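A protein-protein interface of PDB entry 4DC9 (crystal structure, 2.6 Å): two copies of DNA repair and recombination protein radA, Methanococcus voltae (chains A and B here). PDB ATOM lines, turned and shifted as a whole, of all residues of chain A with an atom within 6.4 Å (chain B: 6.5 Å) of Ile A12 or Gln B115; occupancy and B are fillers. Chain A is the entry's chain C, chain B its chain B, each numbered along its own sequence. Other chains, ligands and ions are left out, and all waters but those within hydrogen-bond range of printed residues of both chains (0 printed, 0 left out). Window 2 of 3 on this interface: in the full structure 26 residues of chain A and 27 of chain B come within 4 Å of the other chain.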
ATOM      1  N   LYS A   9     -17.469  23.317 -36.505  1.00  0.00           N
ATOM      2  CA  LYS A   9     -17.767  23.856 -35.171  1.00  0.00           C
ATOM      3  C   LYS A   9     -16.434  24.071 -34.500  1.00  0.00           C
ATOM      4  O   LYS A   9     -15.650  23.134 -34.373  1.00  0.00           O
ATOM      5  CB  LYS A   9     -18.619  22.875 -34.372  1.00  0.00           C
ATOM      6  CG  LYS A   9     -19.896  22.499 -35.085  1.00  0.00           C
ATOM      7  CD  LYS A   9     -20.396  21.121 -34.706  1.00  0.00           C
ATOM      8  CE  LYS A   9     -20.844  21.084 -33.254  1.00  0.00           C
ATOM      9  NZ  LYS A   9     -21.848  20.013 -33.005  1.00  0.00           N
ATOM     10  N   SER A  10     -16.151  25.301 -34.092  1.00  0.00           N
ATOM     11  CA  SER A  10     -14.893  25.595 -33.416  1.00  0.00           C
ATOM     12  C   SER A  10     -14.816  24.824 -32.095  1.00  0.00           C
ATOM     13  O   SER A  10     -15.813  24.280 -31.621  1.00  0.00           O
ATOM     14  CB  SER A  10     -14.786  27.074 -33.126  1.00  0.00           C
ATOM     15  OG  SER A  10     -15.430  27.332 -31.891  1.00  0.00           O
ATOM     16  N   GLY A  11     -13.632  24.777 -31.503  1.00  0.00           N
ATOM     17  CA  GLY A  11     -13.458  24.088 -30.245  1.00  0.00           C
ATOM     18  C   GLY A  11     -14.383  24.712 -29.223  1.00  0.00           C
ATOM     19  O   GLY A  11     -15.151  24.018 -28.552  1.00  0.00           O
ATOM     20  N   ILE A  12     -14.345  26.033 -29.117  1.00  0.00           N
ATOM     21  CA  ILE A  12     -15.186  26.669 -28.142  1.00  0.00           C
ATOM     22  C   ILE A  12     -16.634  26.318 -28.442  1.00  0.00           C
ATOM     23  O   ILE A  12     -17.343  25.845 -27.560  1.00  0.00           O
ATOM     24  CB  ILE A  12     -14.868  28.173 -27.982  1.00  0.00           C
ATOM     25  CG1 ILE A  12     -13.819  28.337 -26.872  1.00  0.00           C
ATOM     26  CG2 ILE A  12     -16.124  28.997 -27.694  1.00  0.00           C
ATOM     27  CD1 ILE A  12     -13.115  29.677 -26.881  1.00  0.00           C
ATOM     28  N   ASP A  13     -17.055  26.472 -29.690  1.00  0.00           N
ATOM     29  CA  ASP A  13     -18.403  26.049 -30.059  1.00  0.00           C
ATOM     30  C   ASP A  13     -18.783  24.645 -29.536  1.00  0.00           C
ATOM     31  O   ASP A  13     -19.942  24.416 -29.172  1.00  0.00           O
ATOM     32  CB  ASP A  13     -18.611  26.145 -31.570  1.00  0.00           C
ATOM     33  CG  ASP A  13     -19.075  27.519 -32.008  1.00  0.00           C
ATOM     34  OD1 ASP A  13     -20.009  28.043 -31.372  1.00  0.00           O
ATOM     35  OD2 ASP A  13     -18.521  28.068 -32.993  1.00  0.00           O
ATOM     36  N   LEU A  14     -17.811  23.724 -29.486  1.00  0.00           N
ATOM     37  CA  LEU A  14     -18.028  22.378 -28.922  1.00  0.00           C
ATOM     38  C   LEU A  14     -18.384  22.389 -27.430  1.00  0.00           C
ATOM     39  O   LEU A  14     -19.277  21.645 -26.999  1.00  0.00           O
ATOM     40  CB  LEU A  14     -16.801  21.484 -29.114  1.00  0.00           C
ATOM     41  CG  LEU A  14     -16.343  21.020 -30.487  1.00  0.00           C
ATOM     42  CD1 LEU A  14     -15.486  19.787 -30.263  1.00  0.00           C
ATOM     43  CD2 LEU A  14     -17.546  20.674 -31.335  1.00  0.00           C
ATOM     44  N   LEU A  15     -17.659  23.198 -26.649  1.00  0.00           N
ATOM     45  CA  LEU A  15     -17.952  23.371 -25.225  1.00  0.00           C
ATOM     46  C   LEU A  15     -19.342  23.982 -25.019  1.00  0.00           C
ATOM     47  O   LEU A  15     -20.169  23.429 -24.297  1.00  0.00           O
ATOM     48  CB  LEU A  15     -16.880  24.231 -24.557  1.00  0.00           C
ATOM     49  CG  LEU A  15     -15.449  23.703 -24.575  1.00  0.00           C
ATOM     50  CD1 LEU A  15     -14.515  24.557 -23.734  1.00  0.00           C
ATOM     51  CD2 LEU A  15     -15.396  22.260 -24.104  1.00  0.00           C
ATOM     52  N   LYS A  16     -19.589  25.112 -25.682  1.00  0.00           N
ATOM     53  CA  LYS A  16     -20.890  25.786 -25.657  1.00  0.00           C
ATOM     54  C   LYS A  16     -21.981  24.823 -26.108  1.00  0.00           C
ATOM     55  O   LYS A  16     -23.085  24.831 -25.565  1.00  0.00           O
ATOM     56  CB  LYS A  16     -20.890  27.070 -26.521  1.00  0.00           C
ATOM     57  CG  LYS A  16     -19.544  27.791 -26.570  1.00  0.00           C
ATOM     58  CD  LYS A  16     -19.594  29.288 -26.266  1.00  0.00           C
ATOM     59  CE  LYS A  16     -18.492  29.637 -25.254  1.00  0.00           C
ATOM     60  NZ  LYS A  16     -17.843  30.969 -25.421  1.00  0.00           N
ATOM     61  N   GLN A  17     -21.664  23.990 -27.095  1.00  0.00           N
ATOM     62  CA  GLN A  17     -22.511  22.869 -27.477  1.00  0.00           C
ATOM     63  C   GLN A  17     -22.844  21.979 -26.252  1.00  0.00           C
ATOM     64  O   GLN A  17     -24.017  21.719 -25.949  1.00  0.00           O
ATOM     65  CB  GLN A  17     -21.806  22.064 -28.581  1.00  0.00           C
ATOM     66  CG  GLN A  17     -22.712  21.315 -29.548  1.00  0.00           C
ATOM     67  CD  GLN A  17     -23.700  22.222 -30.267  1.00  0.00           C
ATOM     68  OE1 GLN A  17     -24.895  21.915 -30.352  1.00  0.00           O
ATOM     69  NE2 GLN A  17     -23.208  23.344 -30.784  1.00  0.00           N
ATOM     70  N   ILE B 103      -6.880  19.314 -25.350  1.00  0.00           N
ATOM     71  CA  ILE B 103      -6.459  20.606 -25.895  1.00  0.00           C
ATOM     72  C   ILE B 103      -6.132  21.544 -24.727  1.00  0.00           C
ATOM     73  O   ILE B 103      -5.030  22.142 -24.666  1.00  0.00           O
ATOM     74  CB  ILE B 103      -7.525  21.216 -26.828  1.00  0.00           C
ATOM     75  CG1 ILE B 103      -7.451  20.563 -28.223  1.00  0.00           C
ATOM     76  CG2 ILE B 103      -7.388  22.731 -26.901  1.00  0.00           C
ATOM     77  CD1 ILE B 103      -6.215  20.912 -29.055  1.00  0.00           C
ATOM     78  N   MET B 104      -7.100  21.614 -23.798  1.00  0.00           N
ATOM     79  CA  MET B 104      -7.007  22.423 -22.597  1.00  0.00           C
ATOM     80  C   MET B 104      -5.738  22.046 -21.838  1.00  0.00           C
ATOM     81  O   MET B 104      -4.839  22.886 -21.634  1.00  0.00           O
ATOM     82  CB  MET B 104      -8.262  22.262 -21.723  1.00  0.00           C
ATOM     83  CG  MET B 104      -9.513  23.041 -22.151  1.00  0.00           C
ATOM     84  SD  MET B 104      -9.306  24.759 -22.722  1.00  0.00           S
ATOM     85  CE  MET B 104      -8.381  25.586 -21.409  1.00  0.00           C
ATOM     86  N   ALA B 107      -2.479  22.813 -23.401  1.00  0.00           N
ATOM     87  CA  ALA B 107      -2.366  24.275 -23.533  1.00  0.00           C
ATOM     88  C   ALA B 107      -1.959  24.956 -22.224  1.00  0.00           C
ATOM     89  O   ALA B 107      -1.058  25.811 -22.219  1.00  0.00           O
ATOM     90  CB  ALA B 107      -3.661  24.872 -24.078  1.00  0.00           C
ATOM     91  N   ILE B 112      -0.073  28.843 -22.310  1.00  0.00           N
ATOM     92  CA  ILE B 112      -0.934  29.416 -23.346  1.00  0.00           C
ATOM     93  C   ILE B 112      -2.351  29.099 -22.911  1.00  0.00           C
ATOM     94  O   ILE B 112      -2.592  28.068 -22.298  1.00  0.00           O
ATOM     95  CB  ILE B 112      -0.654  28.816 -24.768  1.00  0.00           C
ATOM     96  CG1 ILE B 112       0.554  29.509 -25.443  1.00  0.00           C
ATOM     97  CG2 ILE B 112      -1.892  28.847 -25.681  1.00  0.00           C
ATOM     98  CD1 ILE B 112       0.500  31.039 -25.533  1.00  0.00           C
ATOM     99  N   ASP B 113      -3.286  29.982 -23.223  1.00  0.00           N
ATOM    100  CA  ASP B 113      -4.660  29.719 -22.869  1.00  0.00           C
ATOM    101  C   ASP B 113      -5.371  28.798 -23.879  1.00  0.00           C
ATOM    102  O   ASP B 113      -5.426  29.093 -25.082  1.00  0.00           O
ATOM    103  CB  ASP B 113      -5.426  31.022 -22.711  1.00  0.00           C
ATOM    104  CG  ASP B 113      -6.905  30.808 -22.810  1.00  0.00           C
ATOM    105  OD1 ASP B 113      -7.458  30.017 -22.014  1.00  0.00           O
ATOM    106  OD2 ASP B 113      -7.507  31.386 -23.725  1.00  0.00           O
ATOM    107  N   GLY B 114      -5.941  27.707 -23.370  1.00  0.00           N
ATOM    108  CA  GLY B 114      -6.529  26.663 -24.205  1.00  0.00           C
ATOM    109  C   GLY B 114      -7.807  27.105 -24.867  1.00  0.00           C
ATOM    110  O   GLY B 114      -8.124  26.700 -26.004  1.00  0.00           O
ATOM    111  N   GLN B 115      -8.543  27.932 -24.129  1.00  0.00           N
ATOM    112  CA  GLN B 115      -9.761  28.564 -24.606  1.00  0.00           C
ATOM    113  C   GLN B 115      -9.490  29.257 -25.944  1.00  0.00           C
ATOM    114  O   GLN B 115     -10.281  29.138 -26.879  1.00  0.00           O
ATOM    115  CB  GLN B 115     -10.250  29.581 -23.573  1.00  0.00           C
ATOM    116  CG  GLN B 115     -11.729  29.492 -23.210  1.00  0.00           C
ATOM    117  CD  GLN B 115     -12.008  28.526 -22.065  1.00  0.00           C
ATOM    118  OE1 GLN B 115     -13.168  28.238 -21.748  1.00  0.00           O
ATOM    119  NE2 GLN B 115     -10.945  28.022 -21.435  1.00  0.00           N
ATOM    120  N   THR B 116      -8.363  29.969 -26.016  1.00  0.00           N
ATOM    121  CA  THR B 116      -7.897  30.641 -27.233  1.00  0.00           C
ATOM    122  C   THR B 116      -7.765  29.663 -28.385  1.00  0.00           C
ATOM    123  O   THR B 116      -8.262  29.928 -29.489  1.00  0.00           O
ATOM    124  CB  THR B 116      -6.535  31.342 -26.994  1.00  0.00           C
ATOM    125  OG1 THR B 116      -6.775  32.678 -26.551  1.00  0.00           O
ATOM    126  CG2 THR B 116      -5.649  31.377 -28.259  1.00  0.00           C
ATOM    127  N   VAL B 117      -7.089  28.547 -28.091  1.00  0.00           N
ATOM    128  CA  VAL B 117      -6.828  27.481 -29.037  1.00  0.00           C
ATOM    129  C   VAL B 117      -8.159  26.993 -29.588  1.00  0.00           C
ATOM    130  O   VAL B 117      -8.344  26.968 -30.812  1.00  0.00           O
ATOM    131  CB  VAL B 117      -6.004  26.346 -28.390  1.00  0.00           C
ATOM    132  CG1 VAL B 117      -5.904  25.140 -29.308  1.00  0.00           C
ATOM    133  CG2 VAL B 117      -4.609  26.836 -28.030  1.00  0.00           C
ATOM    134  N   LEU B 118      -9.089  26.656 -28.693  1.00  0.00           N
ATOM    135  CA  LEU B 118     -10.431  26.209 -29.089  1.00  0.00           C
ATOM    136  C   LEU B 118     -11.175  27.219 -29.971  1.00  0.00           C
ATOM    137  O   LEU B 118     -12.060  26.860 -30.759  1.00  0.00           O
ATOM    138  CB  LEU B 118     -11.259  25.886 -27.852  1.00  0.00           C
ATOM    139  CG  LEU B 118     -10.660  24.762 -27.021  1.00  0.00           C
ATOM    140  CD1 LEU B 118     -11.259  24.758 -25.618  1.00  0.00           C
ATOM    141  CD2 LEU B 118     -10.894  23.439 -27.734  1.00  0.00           C
ATOM    142  N   ASP B 119     -10.806  28.488 -29.832  1.00  0.00           N
ATOM    143  CA  ASP B 119     -11.437  29.552 -30.595  1.00  0.00           C
ATOM    144  C   ASP B 119     -10.765  29.673 -31.955  1.00  0.00           C
ATOM    145  O   ASP B 119     -11.405  30.014 -32.949  1.00  0.00           O
ATOM    146  CB  ASP B 119     -11.379  30.884 -29.826  1.00  0.00           C
ATOM    147  CG  ASP B 119     -12.677  31.703 -29.955  1.00  0.00           C
ATOM    148  OD1 ASP B 119     -12.574  32.938 -30.052  1.00  0.00           O
ATOM    149  OD2 ASP B 119     -13.797  31.127 -29.971  1.00  0.00           O
ATOM    150  N   ASN B 120      -9.473  29.374 -31.978  1.00  0.00           N
ATOM    151  CA  ASN B 120      -8.719  29.343 -33.210  1.00  0.00           C
ATOM    152  C   ASN B 120      -8.579  27.941 -33.828  1.00  0.00           C
ATOM    153  O   ASN B 120      -7.663  27.702 -34.632  1.00  0.00           O
ATOM    154  CB  ASN B 120      -7.365  30.008 -32.996  1.00  0.00           C
ATOM    155  CG  ASN B 120      -7.501  31.499 -32.761  1.00  0.00           C
ATOM    156  OD1 ASN B 120      -8.445  31.950 -32.103  1.00  0.00           O
ATOM    157  ND2 ASN B 120      -6.575  32.276 -33.320  1.00  0.00           N
ATOM    158  N   THR B 121      -9.485  27.026 -33.463  1.00  0.00           N
ATOM    159  CA  THR B 121      -9.465  25.663 -34.012  1.00  0.00           C
ATOM    160  C   THR B 121     -10.831  25.162 -34.442  1.00  0.00           C
ATOM    161  O   THR B 121     -11.724  24.953 -33.615  1.00  0.00           O
ATOM    162  CB  THR B 121      -8.827  24.667 -33.050  1.00  0.00           C
ATOM    163  OG1 THR B 121      -7.481  25.083 -32.792  1.00  0.00           O
ATOM    164  CG2 THR B 121      -8.807  23.284 -33.660  1.00  0.00           C
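Ile A12 touches just these residues of chain B: Gln B115, Leu B118 and Asp B119. Gln B115 touches just one residue of chain A: Ile A12. Of the printed residues of chain A, Leu B118 touches Ser A10, Gly A11, Ile A12 and Leu A15. Of the printed residues of chain A, Asp B119 touches Ile A12. Printed residues of chain B within 4 Å of Ser A10: Leu B118 (3.6 Å) and Thr B121 (3.2 Å). Printed residues of chain B within 4 Å of Leu A15: Leu B118. Printed residues of chain B within 4 Å of Gly A11: Leu B118 and Thr B121. Ile B112 touches none of the printed residues of chain A. Leu A14 touches none of the printed residues of chain B. The nearest residue of chain B that does not touch Ile A12 is Thr B116 (4.8 Å). The nearest residue of chain A that does not touch Gln B115 is Leu A15 (4.4 Å).
Along chain A the printed residues that touch a printed residue of chain B span positions 10 to 15. Among the printed residues, 8 pairs touch across the chains. Among the printed residues, no Asp or Glu carboxylate lies within 4 Å of a Lys or Arg side-chain nitrogen of the other chain.
The backbone carbonyl oxygen (O) of Leu B118 lies within hydrogen-bond range of the backbone NH (N) of Gly A11, 2.7 Å away. The backbone carbonyl oxygen (O) of Leu B118 sits at hydrogen-bond distance from the backbone NH (N) of Ile A12, at 2.9 Å. The backbone carbonyl oxygen of Thr B121 sits at hydrogen-bond distance from the backbone NH of Gly A11 (2.9 Å).
Ser A10 touches Leu B118. Thr B121 touches Ser A10. Gln B115 touches Ile A12 (O to CD1, 2.9 Å). Asp B119 touches Ile A12. Leu A15 touches Leu B118.
The backbone NH (N) of Gln B115 is in hydrogen-bond range of the side-chain sulfur (SD) of Met B104 (3.6 Å). OD1 of Asp B113 lies within hydrogen-bond range of N of Gln B115. O of Val B117 sits at hydrogen-bond distance from OG1 of Thr B121 (2.9 Å). OG of Ser A10 sits close to N of Ile A12, 3.2 Å away. N of Asp A13 sits at hydrogen-bond distance from OG of Ser A10, 2.9 Å away.
No position is printed for both chains. Of the 8 pairs that touch across the chains among the printed residues, none has its exchanged pair printed and touching as well.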
